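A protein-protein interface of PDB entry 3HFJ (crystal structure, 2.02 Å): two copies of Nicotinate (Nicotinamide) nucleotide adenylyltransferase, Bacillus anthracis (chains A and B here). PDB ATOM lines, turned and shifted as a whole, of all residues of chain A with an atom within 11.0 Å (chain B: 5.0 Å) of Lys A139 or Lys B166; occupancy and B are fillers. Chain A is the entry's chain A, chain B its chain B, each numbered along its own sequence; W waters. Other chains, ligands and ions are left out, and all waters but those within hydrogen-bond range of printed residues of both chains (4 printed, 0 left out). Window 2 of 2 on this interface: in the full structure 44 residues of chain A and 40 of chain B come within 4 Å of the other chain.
The backbone carbonyl oxygen (O) of Lys A139 lies within hydrogen-bond range of the guanidinium group (NH2) of Arg B162. The side-chain amino group of Lys A139 lies close to the side-chain amino group of Lys B166, at 3.4 Å.
The backbone NH (N) of Gly A137 sits at hydrogen-bond distance from the side-chain carboxylate (OE2) of Glu A150, at 2.9 Å. N of Lys B166 sits at hydrogen-bond distance from O of Tyr B189 (2.9 Å).
Among the printed residues, pairs that only touch across the chains: Gly A137 with Glu B163 (3.3 Å), Tyr A138 with Ser B159 (3.5 Å), Lys A139 with Ser B159 (3.4 Å), Lys A139 with Glu B163 (3.5 Å) and Arg A141 with Arg B162 (3.4 Å).
Lys A139 touches just these residues of chain B: Ser B159 (3.4 Å), Arg B162 (3.4 Å), Glu B163 (3.5 Å) and Lys B166 (3.4 Å). Of chain A, only Lys A139 (3.4 Å) comes within 4 Å of Lys B166. Ser B159 touches two residues of chain A. Arg B162 touches just these residues of chain A: Lys A139 (3.4 Å) and Arg A141 (3.4 Å). Of the printed residues of chain A, Glu B163 touches Gly A137 (3.3 Å) and Lys A139 (3.5 Å). Glu B167 touches none of the printed residues of chain A. No residue of chain A comes within 4 Å of Lys B168. No residue of chain A comes within 4 Å of Ser B191. Printed residues of chain B within 4 Å of Gly A137: Glu B163 (3.3 Å). Printed residues of chain B within 4 Å of Arg A141: Arg B162. Printed residues of chain B within 4 Å of Tyr A138: Ser B159. Gly A132 touches none of the printed residues of chain B.
Printed residues of chain A that touch a printed residue of chain B: Gly A137, Tyr A138, Lys A139 and Arg A141. Hydrophobic or aromatic side chains of chain A that line the printed part of chain B: Tyr A138. Of the 11 printed residues of chain B, 4 touch a printed residue of chain A. Among the printed residues, no Asp or Glu carboxylate lies within 4 Å of a Lys or Arg side-chain nitrogen of the other chain.
No position is printed for both chains. Of the 7 pairs that touch across the chains among the printed residues, none has its exchanged pair printed and touching as well.
Water W4 bridges OE2 of Glu B167 (2.6 Å) and O of Gly A137 (3.2 Å). Water W3 lies within hydrogen-bond range of the backbone carbonyl oxygen (O) of Ser B159 (2.8 Å), the backbone NH (N) of Lys A139 (2.9 Å) and the side-chain carboxylate (OE1) of Glu B163 (2.9 Å). Water W2 bridges the guanidinium group (NH2) of Arg B162 (3.0 Å) and the backbone NH (N) of Arg A141 (3.2 Å). Water W1 lies within hydrogen-bond range of N of Tyr B189 (3.0 Å) and NH2 of Arg A141 (3.4 Å).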
ATOM      1  N   GLY A 108     -19.596 -22.349  -0.241  1.00  0.00           N
ATOM      2  CA  GLY A 108     -19.253 -23.686   0.225  1.00  0.00           C
ATOM      3  C   GLY A 108     -17.825 -23.743   0.725  1.00  0.00           C
ATOM      4  O   GLY A 108     -16.950 -23.016   0.232  1.00  0.00           O
ATOM      5  N   GLY A 109     -17.595 -24.597   1.723  1.00  0.00           N
ATOM      6  CA  GLY A 109     -16.266 -24.790   2.301  1.00  0.00           C
ATOM      7  C   GLY A 109     -15.179 -25.049   1.272  1.00  0.00           C
ATOM      8  O   GLY A 109     -14.089 -24.477   1.375  1.00  0.00           O
ATOM      9  N   ASP A 110     -15.481 -25.899   0.284  1.00  0.00           N
ATOM     10  CA  ASP A 110     -14.553 -26.236  -0.804  1.00  0.00           C
ATOM     11  C   ASP A 110     -14.168 -25.027  -1.656  1.00  0.00           C
ATOM     12  O   ASP A 110     -13.126 -25.030  -2.305  1.00  0.00           O
ATOM     13  CB  ASP A 110     -15.166 -27.282  -1.745  1.00  0.00           C
ATOM     14  CG  ASP A 110     -15.290 -28.654  -1.117  1.00  0.00           C
ATOM     15  OD1 ASP A 110     -15.124 -28.782   0.126  1.00  0.00           O
ATOM     16  OD2 ASP A 110     -15.560 -29.614  -1.883  1.00  0.00           O
ATOM     17  N   MET A 111     -15.033 -24.017  -1.682  1.00  0.00           N
ATOM     18  CA  MET A 111     -14.777 -22.807  -2.462  1.00  0.00           C
ATOM     19  C   MET A 111     -13.715 -21.907  -1.819  1.00  0.00           C
ATOM     20  O   MET A 111     -13.041 -21.144  -2.507  1.00  0.00           O
ATOM     21  CB  MET A 111     -16.077 -22.013  -2.661  1.00  0.00           C
ATOM     22  CG  MET A 111     -17.257 -22.858  -3.121  1.00  0.00           C
ATOM     23  SD  MET A 111     -16.833 -23.816  -4.590  1.00  0.00           S
ATOM     24  CE  MET A 111     -16.986 -22.580  -5.854  1.00  0.00           C
ATOM     25  N   VAL A 112     -13.557 -22.016  -0.502  1.00  0.00           N
ATOM     26  CA  VAL A 112     -12.735 -21.049   0.258  1.00  0.00           C
ATOM     27  C   VAL A 112     -11.279 -21.039  -0.214  1.00  0.00           C
ATOM     28  O   VAL A 112     -10.659 -19.975  -0.380  1.00  0.00           O
ATOM     29  CB  VAL A 112     -12.843 -21.323   1.784  1.00  0.00           C
ATOM     30  CG1 VAL A 112     -11.896 -20.453   2.580  1.00  0.00           C
ATOM     31  CG2 VAL A 112     -14.270 -21.099   2.249  1.00  0.00           C
ATOM     32  N   GLU A 113     -10.742 -22.235  -0.450  1.00  0.00           N
ATOM     33  CA  GLU A 113      -9.372 -22.398  -0.931  1.00  0.00           C
ATOM     34  C   GLU A 113      -9.073 -21.618  -2.232  1.00  0.00           C
ATOM     35  O   GLU A 113      -7.921 -21.260  -2.493  1.00  0.00           O
ATOM     36  CB  GLU A 113      -9.069 -23.904  -1.063  1.00  0.00           C
ATOM     37  CG  GLU A 113      -8.164 -24.340  -2.181  1.00  0.00           C
ATOM     38  CD  GLU A 113      -7.928 -25.842  -2.174  1.00  0.00           C
ATOM     39  OE1 GLU A 113      -8.871 -26.623  -1.910  1.00  0.00           O
ATOM     40  OE2 GLU A 113      -6.789 -26.236  -2.436  1.00  0.00           O
ATOM     41  N   GLY A 132     -18.245 -18.827   5.077  1.00  0.00           N
ATOM     42  CA  GLY A 132     -17.918 -20.153   4.600  1.00  0.00           C
ATOM     43  C   GLY A 132     -18.648 -21.208   5.407  1.00  0.00           C
ATOM     44  O   GLY A 132     -18.784 -21.087   6.625  1.00  0.00           O
ATOM     45  N   VAL A 133     -19.099 -22.255   4.725  1.00  0.00           N
ATOM     46  CA  VAL A 133     -19.835 -23.336   5.369  1.00  0.00           C
ATOM     47  C   VAL A 133     -18.871 -24.497   5.635  1.00  0.00           C
ATOM     48  O   VAL A 133     -18.243 -25.021   4.709  1.00  0.00           O
ATOM     49  CB  VAL A 133     -21.044 -23.776   4.507  1.00  0.00           C
ATOM     50  CG1 VAL A 133     -21.638 -25.087   5.021  1.00  0.00           C
ATOM     51  CG2 VAL A 133     -22.101 -22.661   4.484  1.00  0.00           C
ATOM     52  N   ALA A 134     -18.721 -24.855   6.907  1.00  0.00           N
ATOM     53  CA  ALA A 134     -17.868 -25.976   7.292  1.00  0.00           C
ATOM     54  C   ALA A 134     -18.722 -27.076   7.907  1.00  0.00           C
ATOM     55  O   ALA A 134     -19.753 -26.791   8.519  1.00  0.00           O
ATOM     56  CB  ALA A 134     -16.788 -25.516   8.284  1.00  0.00           C
ATOM     57  N   ARG A 135     -18.293 -28.328   7.742  1.00  0.00           N
ATOM     58  CA  ARG A 135     -18.876 -29.440   8.492  1.00  0.00           C
ATOM     59  C   ARG A 135     -18.585 -29.197   9.977  1.00  0.00           C
ATOM     60  O   ARG A 135     -17.551 -28.615  10.317  1.00  0.00           O
ATOM     61  CB  ARG A 135     -18.287 -30.782   8.035  1.00  0.00           C
ATOM     62  CG  ARG A 135     -18.473 -31.102   6.564  1.00  0.00           C
ATOM     63  CD  ARG A 135     -18.536 -32.597   6.329  1.00  0.00           C
ATOM     64  NE  ARG A 135     -18.070 -32.981   4.999  1.00  0.00           N
ATOM     65  CZ  ARG A 135     -18.352 -34.141   4.405  1.00  0.00           C
ATOM     66  NH1 ARG A 135     -19.121 -35.044   5.011  1.00  0.00           N
ATOM     67  NH2 ARG A 135     -17.877 -34.395   3.193  1.00  0.00           N
ATOM     68  N   PRO A 136     -19.502 -29.611  10.872  1.00  0.00           N
ATOM     69  CA  PRO A 136     -19.295 -29.298  12.290  1.00  0.00           C
ATOM     70  C   PRO A 136     -17.986 -29.877  12.813  1.00  0.00           C
ATOM     71  O   PRO A 136     -17.662 -31.029  12.512  1.00  0.00           O
ATOM     72  CB  PRO A 136     -20.504 -29.943  12.972  1.00  0.00           C
ATOM     73  CG  PRO A 136     -21.551 -29.998  11.888  1.00  0.00           C
ATOM     74  CD  PRO A 136     -20.759 -30.349  10.657  1.00  0.00           C
ATOM     75  N   GLY A 137     -17.225 -29.059  13.538  1.00  0.00           N
ATOM     76  CA  GLY A 137     -15.921 -29.462  14.070  1.00  0.00           C
ATOM     77  C   GLY A 137     -14.738 -29.249  13.135  1.00  0.00           C
ATOM     78  O   GLY A 137     -13.597 -29.433  13.542  1.00  0.00           O
ATOM     79  N   TYR A 138     -15.010 -28.874  11.884  1.00  0.00           N
ATOM     80  CA  TYR A 138     -13.972 -28.638  10.869  1.00  0.00           C
ATOM     81  C   TYR A 138     -13.736 -27.135  10.694  1.00  0.00           C
ATOM     82  O   TYR A 138     -14.652 -26.325  10.873  1.00  0.00           O
ATOM     83  CB  TYR A 138     -14.385 -29.219   9.505  1.00  0.00           C
ATOM     84  CG  TYR A 138     -14.656 -30.714   9.436  1.00  0.00           C
ATOM     85  CD1 TYR A 138     -13.978 -31.517   8.515  1.00  0.00           C
ATOM     86  CD2 TYR A 138     -15.614 -31.320  10.253  1.00  0.00           C
ATOM     87  CE1 TYR A 138     -14.228 -32.894   8.424  1.00  0.00           C
ATOM     88  CE2 TYR A 138     -15.876 -32.694  10.175  1.00  0.00           C
ATOM     89  CZ  TYR A 138     -15.175 -33.475   9.260  1.00  0.00           C
ATOM     90  OH  TYR A 138     -15.435 -34.837   9.177  1.00  0.00           O
ATOM     91  N   LYS A 139     -12.518 -26.753  10.322  1.00  0.00           N
ATOM     92  CA  LYS A 139     -12.237 -25.336  10.134  1.00  0.00           C
ATOM     93  C   LYS A 139     -11.691 -25.026   8.748  1.00  0.00           C
ATOM     94  O   LYS A 139     -11.116 -25.881   8.070  1.00  0.00           O
ATOM     95  CB  LYS A 139     -11.359 -24.788  11.276  1.00  0.00           C
ATOM     96  CG  LYS A 139     -11.978 -25.122  12.640  1.00  0.00           C
ATOM     97  CD  LYS A 139     -11.189 -24.677  13.837  1.00  0.00           C
ATOM     98  CE  LYS A 139     -11.699 -25.429  15.067  1.00  0.00           C
ATOM     99  NZ  LYS A 139     -11.438 -24.675  16.330  1.00  0.00           N
ATOM    100  N   LEU A 140     -11.922 -23.793   8.331  1.00  0.00           N
ATOM    101  CA  LEU A 140     -11.549 -23.329   7.014  1.00  0.00           C
ATOM    102  C   LEU A 140     -10.227 -22.591   7.142  1.00  0.00           C
ATOM    103  O   LEU A 140     -10.002 -21.864   8.123  1.00  0.00           O
ATOM    104  CB  LEU A 140     -12.647 -22.421   6.447  1.00  0.00           C
ATOM    105  CG  LEU A 140     -14.043 -23.069   6.428  1.00  0.00           C
ATOM    106  CD1 LEU A 140     -15.133 -22.057   6.115  1.00  0.00           C
ATOM    107  CD2 LEU A 140     -14.073 -24.216   5.456  1.00  0.00           C
ATOM    108  N   ARG A 141      -9.364 -22.798   6.158  1.00  0.00           N
ATOM    109  CA  ARG A 141      -8.045 -22.199   6.147  1.00  0.00           C
ATOM    110  C   ARG A 141      -7.963 -21.221   4.990  1.00  0.00           C
ATOM    111  O   ARG A 141      -8.072 -21.612   3.830  1.00  0.00           O
ATOM    112  CB  ARG A 141      -6.978 -23.290   6.011  1.00  0.00           C
ATOM    113  CG  ARG A 141      -5.575 -22.828   6.357  1.00  0.00           C
ATOM    114  CD  ARG A 141      -4.802 -23.945   6.996  1.00  0.00           C
ATOM    115  NE  ARG A 141      -3.389 -23.641   7.186  1.00  0.00           N
ATOM    116  CZ  ARG A 141      -2.766 -23.654   8.361  1.00  0.00           C
ATOM    117  NH1 ARG A 141      -3.429 -23.946   9.472  1.00  0.00           N
ATOM    118  NH2 ARG A 141      -1.469 -23.378   8.421  1.00  0.00           N
ATOM    119  N   THR A 142      -7.784 -19.946   5.319  1.00  0.00           N
ATOM    120  CA  THR A 142      -7.696 -18.881   4.322  1.00  0.00           C
ATOM    121  C   THR A 142      -6.984 -17.673   4.935  1.00  0.00           C
ATOM    122  O   THR A 142      -7.150 -17.407   6.138  1.00  0.00           O
ATOM    123  CB  THR A 142      -9.115 -18.472   3.770  1.00  0.00           C
ATOM    124  OG1 THR A 142      -9.001 -17.336   2.902  1.00  0.00           O
ATOM    125  CG2 THR A 142     -10.096 -18.136   4.904  1.00  0.00           C
ATOM    126  N   PRO A 143      -6.180 -16.951   4.124  1.00  0.00           N
ATOM    127  CA  PRO A 143      -5.601 -15.667   4.539  1.00  0.00           C
ATOM    128  C   PRO A 143      -6.621 -14.539   4.734  1.00  0.00           C
ATOM    129  O   PRO A 143      -6.283 -13.488   5.332  1.00  0.00           O
ATOM    130  CB  PRO A 143      -4.660 -15.320   3.383  1.00  0.00           C
ATOM    131  CG  PRO A 143      -5.202 -16.037   2.217  1.00  0.00           C
ATOM    132  CD  PRO A 143      -5.738 -17.324   2.765  1.00  0.00           C
ATOM    133  N   TYR A 144      -7.836 -14.735   4.218  1.00  0.00           N
ATOM    134  CA  TYR A 144      -8.879 -13.711   4.292  1.00  0.00           C
ATOM    135  C   TYR A 144      -9.708 -13.837   5.561  1.00  0.00           C
ATOM    136  O   TYR A 144      -9.903 -14.961   6.055  1.00  0.00           O
ATOM    137  CB  TYR A 144      -9.784 -13.783   3.053  1.00  0.00           C
ATOM    138  CG  TYR A 144      -9.019 -13.673   1.750  1.00  0.00           C
ATOM    139  CD1 TYR A 144      -9.302 -14.515   0.678  1.00  0.00           C
ATOM    140  CD2 TYR A 144      -8.000 -12.727   1.596  1.00  0.00           C
ATOM    141  CE1 TYR A 144      -8.601 -14.406  -0.514  1.00  0.00           C
ATOM    142  CE2 TYR A 144      -7.290 -12.625   0.417  1.00  0.00           C
ATOM    143  CZ  TYR A 144      -7.594 -13.464  -0.631  1.00  0.00           C
ATOM    144  OH  TYR A 144      -6.881 -13.341  -1.797  1.00  0.00           O
ATOM    145  N   ILE A 146     -12.840 -14.478   7.206  1.00  0.00           N
ATOM    146  CA  ILE A 146     -14.157 -14.995   6.849  1.00  0.00           C
ATOM    147  C   ILE A 146     -14.877 -15.447   8.108  1.00  0.00           C
ATOM    148  O   ILE A 146     -14.247 -15.719   9.131  1.00  0.00           O
ATOM    149  CB  ILE A 146     -14.106 -16.141   5.766  1.00  0.00           C
ATOM    150  CG1 ILE A 146     -13.469 -17.411   6.324  1.00  0.00           C
ATOM    151  CG2 ILE A 146     -13.375 -15.666   4.488  1.00  0.00           C
ATOM    152  CD1 ILE A 146     -13.751 -18.675   5.443  1.00  0.00           C
ATOM    153  N   THR A 147     -16.201 -15.482   8.030  1.00  0.00           N
ATOM    154  CA  THR A 147     -17.032 -16.047   9.078  1.00  0.00           C
ATOM    155  C   THR A 147     -17.296 -17.507   8.718  1.00  0.00           C
ATOM    156  O   THR A 147     -17.473 -17.855   7.552  1.00  0.00           O
ATOM    157  CB  THR A 147     -18.362 -15.269   9.200  1.00  0.00           C
ATOM    158  OG1 THR A 147     -18.082 -13.900   9.505  1.00  0.00           O
ATOM    159  CG2 THR A 147     -19.286 -15.866  10.286  1.00  0.00           C
ATOM    160  N   THR A 148     -17.304 -18.361   9.727  1.00  0.00           N
ATOM    161  CA  THR A 148     -17.553 -19.773   9.524  1.00  0.00           C
ATOM    162  C   THR A 148     -18.894 -20.123  10.156  1.00  0.00           C
ATOM    163  O   THR A 148     -19.168 -19.744  11.286  1.00  0.00           O
ATOM    164  CB  THR A 148     -16.394 -20.615  10.118  1.00  0.00           C
ATOM    165  OG1 THR A 148     -15.170 -20.279   9.433  1.00  0.00           O
ATOM    166  CG2 THR A 148     -16.655 -22.091   9.964  1.00  0.00           C
ATOM    167  N   VAL A 149     -19.751 -20.811   9.405  1.00  0.00           N
ATOM    168  CA  VAL A 149     -20.973 -21.392   9.977  1.00  0.00           C
ATOM    169  C   VAL A 149     -20.866 -22.901   9.800  1.00  0.00           C
ATOM    170  O   VAL A 149     -20.504 -23.370   8.718  1.00  0.00           O
ATOM    171  CB  VAL A 149     -22.253 -20.844   9.295  1.00  0.00           C
ATOM    172  CG1 VAL A 149     -23.518 -21.597   9.771  1.00  0.00           C
ATOM    173  CG2 VAL A 149     -22.394 -19.358   9.540  1.00  0.00           C
ATOM    174  N   GLU A 150     -21.134 -23.649  10.869  1.00  0.00           N
ATOM    175  CA  GLU A 150     -21.146 -25.113  10.821  1.00  0.00           C
ATOM    176  C   GLU A 150     -22.497 -25.623  10.355  1.00  0.00           C
ATOM    177  O   GLU A 150     -23.543 -25.248  10.897  1.00  0.00           O
ATOM    178  CB  GLU A 150     -20.811 -25.726  12.186  1.00  0.00           C
ATOM    179  CG  GLU A 150     -19.450 -25.315  12.734  1.00  0.00           C
ATOM    180  CD  GLU A 150     -19.058 -26.089  13.987  1.00  0.00           C
ATOM    181  OE1 GLU A 150     -19.965 -26.522  14.743  1.00  0.00           O
ATOM    182  OE2 GLU A 150     -17.841 -26.261  14.206  1.00  0.00           O
ATOM    183  N   ILE A 151     -22.459 -26.484   9.346  1.00  0.00           N
ATOM    184  CA  ILE A 151     -23.647 -27.111   8.781  1.00  0.00           C
ATOM    185  C   ILE A 151     -23.260 -28.542   8.423  1.00  0.00           C
ATOM    186  O   ILE A 151     -22.204 -28.774   7.821  1.00  0.00           O
ATOM    187  CB  ILE A 151     -24.181 -26.377   7.493  1.00  0.00           C
ATOM    188  CG1 ILE A 151     -24.284 -24.860   7.706  1.00  0.00           C
ATOM    189  CG2 ILE A 151     -25.554 -26.928   7.069  1.00  0.00           C
ATOM    190  CD1 ILE A 151     -24.726 -24.062   6.468  1.00  0.00           C
ATOM    191  N   SER B 159      -9.205 -30.142   5.278  1.00  0.00           N
ATOM    192  CA  SER B 159      -9.688 -29.575   6.548  1.00  0.00           C
ATOM    193  C   SER B 159      -9.895 -30.662   7.616  1.00  0.00           C
ATOM    194  O   SER B 159      -9.649 -30.437   8.800  1.00  0.00           O
ATOM    195  CB  SER B 159     -10.975 -28.786   6.348  1.00  0.00           C
ATOM    196  OG  SER B 159     -12.076 -29.662   6.209  1.00  0.00           O
ATOM    197  N   ARG B 162      -6.192 -31.560   8.770  1.00  0.00           N
ATOM    198  CA  ARG B 162      -5.669 -30.453   9.586  1.00  0.00           C
ATOM    199  C   ARG B 162      -6.178 -30.506  11.034  1.00  0.00           C
ATOM    200  O   ARG B 162      -5.404 -30.311  11.978  1.00  0.00           O
ATOM    201  CB  ARG B 162      -5.998 -29.095   8.957  1.00  0.00           C
ATOM    202  CG  ARG B 162      -5.226 -28.793   7.673  1.00  0.00           C
ATOM    203  CD  ARG B 162      -5.347 -27.321   7.273  1.00  0.00           C
ATOM    204  NE  ARG B 162      -6.726 -26.908   7.080  1.00  0.00           N
ATOM    205  CZ  ARG B 162      -7.343 -26.787   5.907  1.00  0.00           C
ATOM    206  NH1 ARG B 162      -6.722 -27.014   4.757  1.00  0.00           N
ATOM    207  NH2 ARG B 162      -8.606 -26.412   5.891  1.00  0.00           N
ATOM    208  N   GLU B 163      -7.472 -30.779  11.195  1.00  0.00           N
ATOM    209  CA  GLU B 163      -8.102 -30.853  12.515  1.00  0.00           C
ATOM    210  C   GLU B 163      -7.605 -32.052  13.322  1.00  0.00           C
ATOM    211  O   GLU B 163      -7.317 -31.937  14.509  1.00  0.00           O
ATOM    212  CB  GLU B 163      -9.634 -30.866  12.378  1.00  0.00           C
ATOM    213  CG  GLU B 163     -10.387 -30.287  13.600  1.00  0.00           C
ATOM    214  CD  GLU B 163      -9.969 -28.852  13.954  1.00  0.00           C
ATOM    215  OE1 GLU B 163      -9.588 -28.066  13.055  1.00  0.00           O
ATOM    216  OE2 GLU B 163     -10.010 -28.508  15.148  1.00  0.00           O
ATOM    217  N   ARG B 164      -7.484 -33.200  12.668  1.00  0.00           N
ATOM    218  CA  ARG B 164      -6.887 -34.383  13.300  1.00  0.00           C
ATOM    219  C   ARG B 164      -5.468 -34.105  13.819  1.00  0.00           C
ATOM    220  O   ARG B 164      -5.143 -34.435  14.963  1.00  0.00           O
ATOM    221  CB  ARG B 164      -6.928 -35.583  12.350  1.00  0.00           C
ATOM    222  CG  ARG B 164      -8.345 -36.061  12.055  1.00  0.00           C
ATOM    223  CD  ARG B 164      -8.379 -37.324  11.195  1.00  0.00           C
ATOM    224  NE  ARG B 164      -7.724 -38.464  11.841  1.00  0.00           N
ATOM    225  CZ  ARG B 164      -8.324 -39.327  12.663  1.00  0.00           C
ATOM    226  NH1 ARG B 164      -9.610 -39.182  12.963  1.00  0.00           N
ATOM    227  NH2 ARG B 164      -7.627 -40.336  13.193  1.00  0.00           N
ATOM    228  N   TYR B 165      -4.626 -33.473  13.002  1.00  0.00           N
ATOM    229  CA  TYR B 165      -3.269 -33.129  13.463  1.00  0.00           C
ATOM    230  C   TYR B 165      -3.234 -32.123  14.634  1.00  0.00           C
ATOM    231  O   TYR B 165      -2.418 -32.250  15.558  1.00  0.00           O
ATOM    232  CB  TYR B 165      -2.401 -32.661  12.303  1.00  0.00           C
ATOM    233  CG  TYR B 165      -1.960 -33.800  11.409  1.00  0.00           C
ATOM    234  CD1 TYR B 165      -2.408 -33.888  10.096  1.00  0.00           C
ATOM    235  CD2 TYR B 165      -1.106 -34.798  11.885  1.00  0.00           C
ATOM    236  CE1 TYR B 165      -2.001 -34.926   9.264  1.00  0.00           C
ATOM    237  CE2 TYR B 165      -0.698 -35.847  11.062  1.00  0.00           C
ATOM    238  CZ  TYR B 165      -1.154 -35.895   9.748  1.00  0.00           C
ATOM    239  OH  TYR B 165      -0.769 -36.918   8.922  1.00  0.00           O
ATOM    240  N   LYS B 166      -4.137 -31.146  14.588  1.00  0.00           N
ATOM    241  CA  LYS B 166      -4.344 -30.209  15.690  1.00  0.00           C
ATOM    242  C   LYS B 166      -4.639 -30.928  17.003  1.00  0.00           C
ATOM    243  O   LYS B 166      -4.118 -30.549  18.053  1.00  0.00           O
ATOM    244  CB  LYS B 166      -5.479 -29.242  15.348  1.00  0.00           C
ATOM    245  CG  LYS B 166      -5.674 -28.097  16.343  1.00  0.00           C
ATOM    246  CD  LYS B 166      -6.779 -27.198  15.833  1.00  0.00           C
ATOM    247  CE  LYS B 166      -6.976 -25.970  16.700  1.00  0.00           C
ATOM    248  NZ  LYS B 166      -8.049 -25.109  16.106  1.00  0.00           N
ATOM    249  N   GLU B 167      -5.463 -31.973  16.922  1.00  0.00           N
ATOM    250  CA  GLU B 167      -5.866 -32.779  18.079  1.00  0.00           C
ATOM    251  C   GLU B 167      -4.896 -33.923  18.354  1.00  0.00           C
ATOM    252  O   GLU B 167      -5.201 -34.837  19.127  1.00  0.00           O
ATOM    253  CB  GLU B 167      -7.270 -33.337  17.854  1.00  0.00           C
ATOM    254  CG  GLU B 167      -8.330 -32.272  17.636  1.00  0.00           C
ATOM    255  CD  GLU B 167      -9.665 -32.860  17.207  1.00  0.00           C
ATOM    256  OE1 GLU B 167      -9.720 -34.075  16.904  1.00  0.00           O
ATOM    257  OE2 GLU B 167     -10.659 -32.109  17.167  1.00  0.00           O
ATOM    258  N   LYS B 168      -3.731 -33.873  17.706  1.00  0.00           N
ATOM    259  CA  LYS B 168      -2.693 -34.890  17.864  1.00  0.00           C
ATOM    260  C   LYS B 168      -3.231 -36.307  17.604  1.00  0.00           C
ATOM    261  O   LYS B 168      -2.859 -37.263  18.287  1.00  0.00           O
ATOM    262  CB  LYS B 168      -2.008 -34.780  19.240  1.00  0.00           C
ATOM    263  CG  LYS B 168      -1.431 -33.393  19.538  1.00  0.00           C
ATOM    264  CD  LYS B 168      -0.506 -33.437  20.745  1.00  0.00           C
ATOM    265  CE  LYS B 168      -0.282 -32.052  21.338  1.00  0.00           C
ATOM    266  NZ  LYS B 168       0.652 -32.107  22.504  1.00  0.00           N
ATOM    267  N   TYR B 189       0.138 -27.913  11.296  1.00  0.00           N
ATOM    268  CA  TYR B 189      -1.303 -28.013  11.589  1.00  0.00           C
ATOM    269  C   TYR B 189      -1.631 -28.322  13.048  1.00  0.00           C
ATOM    270  O   TYR B 189      -2.593 -29.040  13.327  1.00  0.00           O
ATOM    271  CB  TYR B 189      -1.997 -29.049  10.684  1.00  0.00           C
ATOM    272  CG  TYR B 189      -1.693 -28.918   9.212  1.00  0.00           C
ATOM    273  CD1 TYR B 189      -2.010 -27.750   8.515  1.00  0.00           C
ATOM    274  CD2 TYR B 189      -1.091 -29.967   8.508  1.00  0.00           C
ATOM    275  CE1 TYR B 189      -1.736 -27.624   7.159  1.00  0.00           C
ATOM    276  CE2 TYR B 189      -0.801 -29.848   7.148  1.00  0.00           C
ATOM    277  CZ  TYR B 189      -1.138 -28.677   6.483  1.00  0.00           C
ATOM    278  OH  TYR B 189      -0.869 -28.547   5.147  1.00  0.00           O
ATOM    279  N   GLU B 190      -0.842 -27.803  13.982  1.00  0.00           N
ATOM    280  CA  GLU B 190      -1.144 -28.070  15.386  1.00  0.00           C
ATOM    281  C   GLU B 190      -1.324 -26.798  16.202  1.00  0.00           C
ATOM    282  O   GLU B 190      -0.710 -26.621  17.261  1.00  0.00           O
ATOM    283  CB  GLU B 190      -0.169 -29.084  16.012  1.00  0.00           C
ATOM    284  CG  GLU B 190       1.299 -28.684  16.075  1.00  0.00           C
ATOM    285  CD  GLU B 190       2.155 -29.798  16.640  1.00  0.00           C
ATOM    286  OE1 GLU B 190       1.718 -30.969  16.584  1.00  0.00           O
ATOM    287  OE2 GLU B 190       3.267 -29.504  17.142  1.00  0.00           O
ATOM    288  N   SER B 191      -2.204 -25.939  15.692  1.00  0.00           N
ATOM    289  CA  SER B 191      -2.481 -24.610  16.241  1.00  0.00           C
ATOM    290  C   SER B 191      -1.286 -23.681  16.018  1.00  0.00           C
ATOM    291  O   SER B 191      -1.417 -22.627  15.390  1.00  0.00           O
ATOM    292  CB  SER B 191      -2.887 -24.675  17.724  1.00  0.00           C
ATOM    293  OG  SER B 191      -3.804 -25.733  17.983  1.00  0.00           O
HETATM  294  O   HOH W   1       0.599 -25.962   9.011  1.00  0.00           O
HETATM  295  O   HOH W   2     -10.477 -25.012   4.067  1.00  0.00           O
HETATM  296  O   HOH W   3      -9.994 -28.093  10.208  1.00  0.00           O
HETATM  297  O   HOH W   4     -12.879 -31.367  16.036  1.00  0.00           O
